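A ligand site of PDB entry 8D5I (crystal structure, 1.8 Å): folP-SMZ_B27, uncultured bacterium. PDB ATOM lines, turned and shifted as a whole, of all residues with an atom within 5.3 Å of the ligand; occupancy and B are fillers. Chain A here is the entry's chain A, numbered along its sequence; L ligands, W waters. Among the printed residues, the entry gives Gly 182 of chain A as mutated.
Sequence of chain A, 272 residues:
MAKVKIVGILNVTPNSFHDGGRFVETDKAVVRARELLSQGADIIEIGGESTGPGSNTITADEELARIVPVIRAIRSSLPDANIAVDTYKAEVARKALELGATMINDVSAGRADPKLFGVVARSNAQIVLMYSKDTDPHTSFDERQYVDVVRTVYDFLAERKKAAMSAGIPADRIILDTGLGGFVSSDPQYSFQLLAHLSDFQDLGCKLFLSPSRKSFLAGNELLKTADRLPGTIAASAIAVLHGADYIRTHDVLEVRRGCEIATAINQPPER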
ATOM      1  N   GLU A  45     -18.089 -16.660   6.993  1.00  0.00           N
ATOM      2  CA  GLU A  45     -17.776 -18.069   6.746  1.00  0.00           C
ATOM      3  C   GLU A  45     -16.519 -18.444   7.513  1.00  0.00           C
ATOM      4  O   GLU A  45     -15.417 -18.039   7.146  1.00  0.00           O
ATOM      5  CB  GLU A  45     -17.584 -18.345   5.259  1.00  0.00           C
ATOM      6  CG  GLU A  45     -17.213 -19.822   4.982  1.00  0.00           C
ATOM      7  CD  GLU A  45     -16.508 -19.983   3.659  1.00  0.00           C
ATOM      8  OE1 GLU A  45     -17.226 -20.172   2.653  1.00  0.00           O
ATOM      9  OE2 GLU A  45     -15.250 -19.896   3.605  1.00  0.00           O
ATOM     10  N   THR A  51      -7.558 -24.632   2.063  1.00  0.00           N
ATOM     11  CA  THR A  51      -7.400 -25.467   0.875  1.00  0.00           C
ATOM     12  C   THR A  51      -6.700 -24.779  -0.282  1.00  0.00           C
ATOM     13  O   THR A  51      -6.711 -25.319  -1.403  1.00  0.00           O
ATOM     14  CB  THR A  51      -8.777 -26.022   0.429  1.00  0.00           C
ATOM     15  OG1 THR A  51      -9.740 -24.963   0.369  1.00  0.00           O
ATOM     16  CG2 THR A  51      -9.266 -27.065   1.410  1.00  0.00           C
ATOM     17  N   GLY A  52      -6.047 -23.637  -0.069  1.00  0.00           N
ATOM     18  CA  GLY A  52      -5.233 -23.030  -1.093  1.00  0.00           C
ATOM     19  C   GLY A  52      -3.879 -23.695  -1.299  1.00  0.00           C
ATOM     20  O   GLY A  52      -3.612 -24.794  -0.804  1.00  0.00           O
ATOM     21  N   PRO A  53      -2.986 -23.019  -2.055  1.00  0.00           N
ATOM     22  CA  PRO A  53      -1.700 -23.615  -2.451  1.00  0.00           C
ATOM     23  C   PRO A  53      -0.891 -24.181  -1.289  1.00  0.00           C
ATOM     24  O   PRO A  53      -0.582 -23.458  -0.337  1.00  0.00           O
ATOM     25  CB  PRO A  53      -0.951 -22.449  -3.107  1.00  0.00           C
ATOM     26  CG  PRO A  53      -2.016 -21.591  -3.644  1.00  0.00           C
ATOM     27  CD  PRO A  53      -3.223 -21.730  -2.748  1.00  0.00           C
ATOM     28  N   ASP A  86     -16.978 -23.616   6.378  1.00  0.00           N
ATOM     29  CA  ASP A  86     -16.237 -24.204   5.263  1.00  0.00           C
ATOM     30  C   ASP A  86     -15.622 -25.502   5.779  1.00  0.00           C
ATOM     31  O   ASP A  86     -14.580 -25.480   6.438  1.00  0.00           O
ATOM     32  CB  ASP A  86     -15.160 -23.208   4.787  1.00  0.00           C
ATOM     33  CG  ASP A  86     -14.400 -23.667   3.545  1.00  0.00           C
ATOM     34  OD1 ASP A  86     -14.255 -24.891   3.311  1.00  0.00           O
ATOM     35  OD2 ASP A  86     -13.976 -22.800   2.760  1.00  0.00           O
ATOM     36  N   ASN A 105     -20.339 -25.064   3.457  1.00  0.00           N
ATOM     37  CA  ASN A 105     -19.638 -24.917   2.178  1.00  0.00           C
ATOM     38  C   ASN A 105     -18.652 -26.073   2.025  1.00  0.00           C
ATOM     39  O   ASN A 105     -17.645 -26.129   2.726  1.00  0.00           O
ATOM     40  CB  ASN A 105     -18.933 -23.556   2.159  1.00  0.00           C
ATOM     41  CG  ASN A 105     -18.063 -23.343   0.931  1.00  0.00           C
ATOM     42  OD1 ASN A 105     -18.283 -23.957  -0.110  1.00  0.00           O
ATOM     43  ND2 ASN A 105     -17.106 -22.421   1.037  1.00  0.00           N
ATOM     44  N   VAL A 107     -16.056 -28.013  -0.290  1.00  0.00           N
ATOM     45  CA  VAL A 107     -15.234 -27.986  -1.496  1.00  0.00           C
ATOM     46  C   VAL A 107     -15.126 -29.335  -2.170  1.00  0.00           C
ATOM     47  O   VAL A 107     -14.622 -29.401  -3.300  1.00  0.00           O
ATOM     48  CB  VAL A 107     -13.825 -27.434  -1.187  1.00  0.00           C
ATOM     49  CG1 VAL A 107     -13.898 -25.964  -0.764  1.00  0.00           C
ATOM     50  CG2 VAL A 107     -13.146 -28.245  -0.096  1.00  0.00           C
ATOM     51  N   VAL A 128     -23.280 -25.681  -0.089  1.00  0.00           N
ATOM     52  CA  VAL A 128     -22.604 -25.248  -1.304  1.00  0.00           C
ATOM     53  C   VAL A 128     -21.846 -26.457  -1.845  1.00  0.00           C
ATOM     54  O   VAL A 128     -21.037 -27.050  -1.132  1.00  0.00           O
ATOM     55  CB  VAL A 128     -21.645 -24.076  -1.059  1.00  0.00           C
ATOM     56  CG1 VAL A 128     -21.075 -23.574  -2.411  1.00  0.00           C
ATOM     57  CG2 VAL A 128     -22.327 -22.938  -0.297  1.00  0.00           C
ATOM     58  N   MET A 130     -19.274 -27.379  -4.642  1.00  0.00           N
ATOM     59  CA  MET A 130     -18.306 -26.821  -5.582  1.00  0.00           C
ATOM     60  C   MET A 130     -17.656 -27.903  -6.420  1.00  0.00           C
ATOM     61  O   MET A 130     -17.353 -28.997  -5.928  1.00  0.00           O
ATOM     62  CB  MET A 130     -17.267 -25.992  -4.826  1.00  0.00           C
ATOM     63  CG  MET A 130     -16.191 -25.401  -5.751  1.00  0.00           C
ATOM     64  SD  MET A 130     -14.754 -25.019  -4.723  1.00  0.00           S
ATOM     65  CE  MET A 130     -13.736 -26.389  -5.299  1.00  0.00           C
ATOM     66  N   PHE A 141      -2.179 -28.784  -7.640  1.00  0.00           N
ATOM     67  CA  PHE A 141      -2.877 -28.070  -8.711  1.00  0.00           C
ATOM     68  C   PHE A 141      -2.187 -28.345 -10.038  1.00  0.00           C
ATOM     69  O   PHE A 141      -1.334 -27.574 -10.493  1.00  0.00           O
ATOM     70  CB  PHE A 141      -2.945 -26.576  -8.385  1.00  0.00           C
ATOM     71  CG  PHE A 141      -3.807 -26.244  -7.193  1.00  0.00           C
ATOM     72  CD1 PHE A 141      -4.821 -27.106  -6.803  1.00  0.00           C
ATOM     73  CD2 PHE A 141      -3.590 -25.085  -6.446  1.00  0.00           C
ATOM     74  CE1 PHE A 141      -5.625 -26.811  -5.710  1.00  0.00           C
ATOM     75  CE2 PHE A 141      -4.388 -24.789  -5.345  1.00  0.00           C
ATOM     76  CZ  PHE A 141      -5.405 -25.647  -4.979  1.00  0.00           C
ATOM     77  N   ASP A 177     -21.308 -24.022  -7.241  1.00  0.00           N
ATOM     78  CA  ASP A 177     -20.075 -23.275  -7.456  1.00  0.00           C
ATOM     79  C   ASP A 177     -19.284 -24.025  -8.526  1.00  0.00           C
ATOM     80  O   ASP A 177     -19.073 -25.224  -8.398  1.00  0.00           O
ATOM     81  CB  ASP A 177     -19.265 -23.184  -6.134  1.00  0.00           C
ATOM     82  CG  ASP A 177     -18.000 -22.312  -6.234  1.00  0.00           C
ATOM     83  OD1 ASP A 177     -17.439 -22.097  -7.346  1.00  0.00           O
ATOM     84  OD2 ASP A 177     -17.544 -21.838  -5.165  1.00  0.00           O
ATOM     85  N   GLY A 179     -16.219 -23.774  -9.083  1.00  0.00           N
ATOM     86  CA  GLY A 179     -14.799 -23.813  -8.779  1.00  0.00           C
ATOM     87  C   GLY A 179     -14.072 -22.769  -9.610  1.00  0.00           C
ATOM     88  O   GLY A 179     -14.581 -22.359 -10.661  1.00  0.00           O
ATOM     89  N   LEU A 180     -12.926 -22.309  -9.126  1.00  0.00           N
ATOM     90  CA  LEU A 180     -12.084 -21.359  -9.834  1.00  0.00           C
ATOM     91  C   LEU A 180     -10.643 -21.674  -9.454  1.00  0.00           C
ATOM     92  O   LEU A 180     -10.383 -22.387  -8.475  1.00  0.00           O
ATOM     93  CB  LEU A 180     -12.448 -19.902  -9.482  1.00  0.00           C
ATOM     94  CG  LEU A 180     -13.799 -19.373  -9.983  1.00  0.00           C
ATOM     95  CD1 LEU A 180     -14.129 -17.984  -9.417  1.00  0.00           C
ATOM     96  CD2 LEU A 180     -13.812 -19.350 -11.514  1.00  0.00           C
ATOM     97  N   GLY A 181      -9.706 -21.126 -10.230  1.00  0.00           N
ATOM     98  CA  GLY A 181      -8.301 -21.330  -9.922  1.00  0.00           C
ATOM     99  C   GLY A 181      -7.893 -22.796  -9.963  1.00  0.00           C
ATOM    100  O   GLY A 181      -8.350 -23.573 -10.809  1.00  0.00           O
ATOM    101  N   GLY A 182      -6.997 -23.172  -9.043  1.00  0.00           N
ATOM    102  CA  GLY A 182      -6.398 -24.516  -9.048  1.00  0.00           C
ATOM    103  C   GLY A 182      -7.391 -25.652  -8.898  1.00  0.00           C
ATOM    104  O   GLY A 182      -7.078 -26.790  -9.261  1.00  0.00           O
ATOM    105  N   PHE A 183      -8.568 -25.368  -8.333  1.00  0.00           N
ATOM    106  CA  PHE A 183      -9.643 -26.368  -8.261  1.00  0.00           C
ATOM    107  C   PHE A 183     -10.103 -26.810  -9.648  1.00  0.00           C
ATOM    108  O   PHE A 183     -10.623 -27.913  -9.816  1.00  0.00           O
ATOM    109  CB  PHE A 183     -10.830 -25.807  -7.478  1.00  0.00           C
ATOM    110  CG  PHE A 183     -10.634 -25.780  -5.978  1.00  0.00           C
ATOM    111  CD1 PHE A 183     -10.012 -26.835  -5.313  1.00  0.00           C
ATOM    112  CD2 PHE A 183     -11.118 -24.713  -5.222  1.00  0.00           C
ATOM    113  CE1 PHE A 183      -9.867 -26.827  -3.936  1.00  0.00           C
ATOM    114  CE2 PHE A 183     -11.008 -24.713  -3.817  1.00  0.00           C
ATOM    115  CZ  PHE A 183     -10.359 -25.771  -3.185  1.00  0.00           C
ATOM    116  N   PHE A 209     -22.651 -19.497  -6.598  1.00  0.00           N
ATOM    117  CA  PHE A 209     -21.737 -19.029  -5.552  1.00  0.00           C
ATOM    118  C   PHE A 209     -20.338 -19.119  -6.143  1.00  0.00           C
ATOM    119  O   PHE A 209     -19.971 -20.158  -6.679  1.00  0.00           O
ATOM    120  CB  PHE A 209     -21.914 -19.959  -4.333  1.00  0.00           C
ATOM    121  CG  PHE A 209     -20.984 -19.729  -3.164  1.00  0.00           C
ATOM    122  CD1 PHE A 209     -19.618 -19.925  -3.269  1.00  0.00           C
ATOM    123  CD2 PHE A 209     -21.540 -19.472  -1.908  1.00  0.00           C
ATOM    124  CE1 PHE A 209     -18.804 -19.798  -2.146  1.00  0.00           C
ATOM    125  CE2 PHE A 209     -20.727 -19.355  -0.782  1.00  0.00           C
ATOM    126  CZ  PHE A 209     -19.346 -19.506  -0.907  1.00  0.00           C
ATOM    127  N   SER A 211     -15.979 -17.767  -5.794  1.00  0.00           N
ATOM    128  CA  SER A 211     -14.914 -17.221  -4.952  1.00  0.00           C
ATOM    129  C   SER A 211     -13.682 -16.886  -5.779  1.00  0.00           C
ATOM    130  O   SER A 211     -12.661 -17.585  -5.719  1.00  0.00           O
ATOM    131  CB  SER A 211     -14.564 -18.224  -3.844  1.00  0.00           C
ATOM    132  OG  SER A 211     -13.770 -17.647  -2.807  1.00  0.00           O
ATOM    133  N   ARG A 214      -8.615 -13.496  -5.042  1.00  0.00           N
ATOM    134  CA  ARG A 214      -7.167 -13.460  -5.215  1.00  0.00           C
ATOM    135  C   ARG A 214      -6.540 -14.796  -5.571  1.00  0.00           C
ATOM    136  O   ARG A 214      -5.355 -15.033  -5.294  1.00  0.00           O
ATOM    137  CB  ARG A 214      -6.469 -12.845  -3.987  1.00  0.00           C
ATOM    138  CG  ARG A 214      -7.066 -11.491  -3.595  1.00  0.00           C
ATOM    139  CD  ARG A 214      -6.114 -10.820  -2.630  1.00  0.00           C
ATOM    140  NE  ARG A 214      -6.639  -9.622  -1.982  1.00  0.00           N
ATOM    141  CZ  ARG A 214      -5.943  -8.503  -1.859  1.00  0.00           C
ATOM    142  NH1 ARG A 214      -4.749  -8.377  -2.416  1.00  0.00           N
ATOM    143  NH2 ARG A 214      -6.459  -7.477  -1.185  1.00  0.00           N
ATOM    144  N   LYS A 215      -7.284 -15.656  -6.263  1.00  0.00           N
ATOM    145  CA  LYS A 215      -6.746 -16.951  -6.661  1.00  0.00           C
ATOM    146  C   LYS A 215      -5.746 -16.815  -7.807  1.00  0.00           C
ATOM    147  O   LYS A 215      -5.676 -15.795  -8.486  1.00  0.00           O
ATOM    148  CB  LYS A 215      -7.866 -17.911  -7.081  1.00  0.00           C
ATOM    149  CG  LYS A 215      -8.761 -18.404  -5.956  1.00  0.00           C
ATOM    150  CD  LYS A 215      -9.853 -19.300  -6.534  1.00  0.00           C
ATOM    151  CE  LYS A 215     -10.457 -20.191  -5.485  1.00  0.00           C
ATOM    152  NZ  LYS A 215     -10.916 -19.417  -4.287  1.00  0.00           N
ATOM    153  N   SER A 216      -5.032 -17.912  -8.059  1.00  0.00           N
ATOM    154  CA  SER A 216      -3.905 -17.963  -8.998  1.00  0.00           C
ATOM    155  C   SER A 216      -4.300 -17.629 -10.433  1.00  0.00           C
ATOM    156  O   SER A 216      -3.442 -17.165 -11.210  1.00  0.00           O
ATOM    157  CB  SER A 216      -3.264 -19.347  -8.939  1.00  0.00           C
ATOM    158  OG  SER A 216      -4.212 -20.352  -9.288  1.00  0.00           O
ATOM    159  N   PHE A 217      -5.550 -17.875 -10.845  1.00  0.00           N
ATOM    160  CA  PHE A 217      -5.926 -17.513 -12.211  1.00  0.00           C
ATOM    161  C   PHE A 217      -5.942 -16.012 -12.442  1.00  0.00           C
ATOM    162  O   PHE A 217      -5.933 -15.588 -13.602  1.00  0.00           O
ATOM    163  CB  PHE A 217      -7.280 -18.108 -12.641  1.00  0.00           C
ATOM    164  CG  PHE A 217      -8.500 -17.401 -12.090  1.00  0.00           C
ATOM    165  CD1 PHE A 217      -8.916 -17.598 -10.773  1.00  0.00           C
ATOM    166  CD2 PHE A 217      -9.249 -16.550 -12.897  1.00  0.00           C
ATOM    167  CE1 PHE A 217     -10.057 -16.937 -10.270  1.00  0.00           C
ATOM    168  CE2 PHE A 217     -10.372 -15.899 -12.418  1.00  0.00           C
ATOM    169  CZ  PHE A 217     -10.787 -16.085 -11.104  1.00  0.00           C
ATOM    170  N   ARG A 229      -3.501  -8.816  -6.430  1.00  0.00           N
ATOM    171  CA  ARG A 229      -4.635  -9.355  -7.173  1.00  0.00           C
ATOM    172  C   ARG A 229      -5.981  -8.747  -6.798  1.00  0.00           C
ATOM    173  O   ARG A 229      -7.011  -9.261  -7.232  1.00  0.00           O
ATOM    174  CB  ARG A 229      -4.695 -10.876  -7.009  1.00  0.00           C
ATOM    175  CG  ARG A 229      -3.450 -11.603  -7.475  1.00  0.00           C
ATOM    176  CD  ARG A 229      -3.605 -13.119  -7.304  1.00  0.00           C
ATOM    177  NE  ARG A 229      -2.384 -13.823  -7.669  1.00  0.00           N
ATOM    178  CZ  ARG A 229      -2.044 -15.020  -7.222  1.00  0.00           C
ATOM    179  NH1 ARG A 229      -2.809 -15.686  -6.374  1.00  0.00           N
ATOM    180  NH2 ARG A 229      -0.897 -15.568  -7.625  1.00  0.00           N
ATOM    181  N   ARG A 249     -17.769 -14.976  -2.505  1.00  0.00           N
ATOM    182  CA  ARG A 249     -16.930 -15.225  -1.326  1.00  0.00           C
ATOM    183  C   ARG A 249     -15.611 -14.465  -1.457  1.00  0.00           C
ATOM    184  O   ARG A 249     -14.918 -14.593  -2.462  1.00  0.00           O
ATOM    185  CB  ARG A 249     -16.687 -16.735  -1.200  1.00  0.00           C
ATOM    186  CG  ARG A 249     -15.658 -17.178  -0.163  1.00  0.00           C
ATOM    187  CD  ARG A 249     -15.530 -18.723  -0.171  1.00  0.00           C
ATOM    188  NE  ARG A 249     -14.677 -19.205   0.904  1.00  0.00           N
ATOM    189  CZ  ARG A 249     -13.351 -19.206   0.866  1.00  0.00           C
ATOM    190  NH1 ARG A 249     -12.689 -18.766  -0.190  1.00  0.00           N
ATOM    191  NH2 ARG A 249     -12.665 -19.661   1.920  1.00  0.00           N
HETATM  192  C1  LIG L   1     -13.951 -21.710  -3.544  1.00  0.00           C
HETATM  193  C2  LIG L   1     -13.245 -21.923  -2.375  1.00  0.00           C
HETATM  194  C3  LIG L   1     -13.862 -22.370  -1.251  1.00  0.00           C
HETATM  195  N1  LIG L   1     -11.924 -21.663  -2.384  1.00  0.00           N
HETATM  196  C4  LIG L   1     -15.878 -22.414  -2.470  1.00  0.00           C
HETATM  197  N2  LIG L   1     -15.192 -22.604  -1.304  1.00  0.00           N
HETATM  198  C5  LIG L   1     -11.208 -21.838  -1.294  1.00  0.00           C
HETATM  199  N3  LIG L   1     -17.257 -22.764  -2.223  1.00  0.00           N
HETATM  200  C6  LIG L   1     -11.814 -22.290  -0.114  1.00  0.00           C
HETATM  201  C7  LIG L   1      -5.638 -20.828  -6.249  1.00  0.00           C
HETATM  202  O1  LIG L   1      -5.628 -21.477  -7.339  1.00  0.00           O
HETATM  203  O2  LIG L   1     -13.332 -21.291  -4.689  1.00  0.00           O
HETATM  204  N4  LIG L   1     -15.246 -21.945  -3.584  1.00  0.00           N
HETATM  205  N5  LIG L   1     -13.133 -22.531  -0.110  1.00  0.00           N
HETATM  206  C8  LIG L   1      -9.711 -21.646  -0.991  1.00  0.00           C
HETATM  207  N6  LIG L   1      -8.986 -22.581  -1.864  1.00  0.00           N
HETATM  208  C9  LIG L   1      -8.126 -22.143  -2.977  1.00  0.00           C
HETATM  209  C10 LIG L   1      -7.964 -22.948  -4.099  1.00  0.00           C
HETATM  210  C11 LIG L   1      -7.483 -20.917  -2.911  1.00  0.00           C
HETATM  211  C12 LIG L   1      -7.160 -22.551  -5.163  1.00  0.00           C
HETATM  212  C13 LIG L   1      -6.673 -20.505  -3.957  1.00  0.00           C
HETATM  213  C14 LIG L   1      -6.512 -21.310  -5.079  1.00  0.00           C
HETATM  214  O3  LIG L   1      -4.958 -19.763  -6.141  1.00  0.00           O
HETATM  215  O   HOH W   1     -15.179 -20.396  -6.959  1.00  0.00           O
HETATM  216  O   HOH W   2      -6.639 -17.210  -3.074  1.00  0.00           O
HETATM  217  O   HOH W   3      -9.360 -18.027  -2.637  1.00  0.00           O
HETATM  218  O   HOH W   4      -2.583 -18.345  -5.519  1.00  0.00           O
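Water W4 bridges NH1 of Arg 229 (2.8 Å) and O3 of the ligand (2.8 Å). Water W1 lies within hydrogen-bond range of the side-chain carboxylate of Asp 177 (2.9 Å), the backbone NH of Ser 211 (3.0 Å) and an oxygen (O2) of the ligand (3.1 Å).
OD2 of Asp 86 lies close to N5 of the ligand (3.0 Å). A nitrogen (N4) of the ligand lies close to the side-chain sulfur (SD) of Met 130, 3.3 Å away. CA of Gly 52 touches C9 of the ligand (3.6 Å). Pro 53 touches the ligand. Val 107 touches the ligand. CG1 of Val 128 touches N3 of the ligand, 3.9 Å away. Phe 141 touches the ligand. Gly 181 touches the ligand. Phe 183 touches the ligand. Phe 209 touches the ligand. Ser 211 touches the ligand. Arg 249 touches the ligand (NH2 to C6, 3.4 Å). Hydrophobic or aromatic side chains within 4 Å of the ligand: Pro 53, Val 107, Val 128, Met 130, Phe 141, Phe 183 and Phe 209. Of the 24 residues printed, 18 come within 4 Å of the ligand.
An oxygen (O1) of the ligand is in hydrogen-bond range of the backbone NH (N) of Gly 182. N of Ser 216 is in hydrogen-bond range of O3 of the ligand, 2.7 Å away. The side-chain amino group of Lys 215 is in hydrogen-bond range of an oxygen (O2) of the ligand, at 3.1 Å. OG of Ser 216 lies within hydrogen-bond range of O1 of the ligand (2.7 Å). N6 of the ligand lies within hydrogen-bond range of OG1 of Thr 51, 3.4 Å away. N4 of the ligand sits at hydrogen-bond distance from OD2 of Asp 177 (2.8 Å). OD1 of Asn 105 lies within hydrogen-bond range of N3 of the ligand (2.6 Å).
The side-chain amino group (NZ) of Lys 215 is in hydrogen-bond range of the backbone carbonyl oxygen (O) of Ser 211 (2.9 Å). The side-chain carboxylate of Asp 177 lies within hydrogen-bond range of the backbone NH of Gly 179 (2.7 Å). The guanidinium group (NE) of Arg 249 is in salt-bridge range of the side-chain carboxylate (OE2) of Glu 45 (2.8 Å). The guanidinium group (NH2) of Arg 249 is in salt-bridge range of the side-chain carboxylate (OD2) of Asp 86, 3.5 Å away. OE1 of Glu 45 sits at hydrogen-bond distance from ND2 of Asn 105 (2.8 Å). The side-chain hydroxyl (OG) of Ser 211 sits at hydrogen-bond distance from the guanidinium group (NH1) of Arg 249 (3.0 Å).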
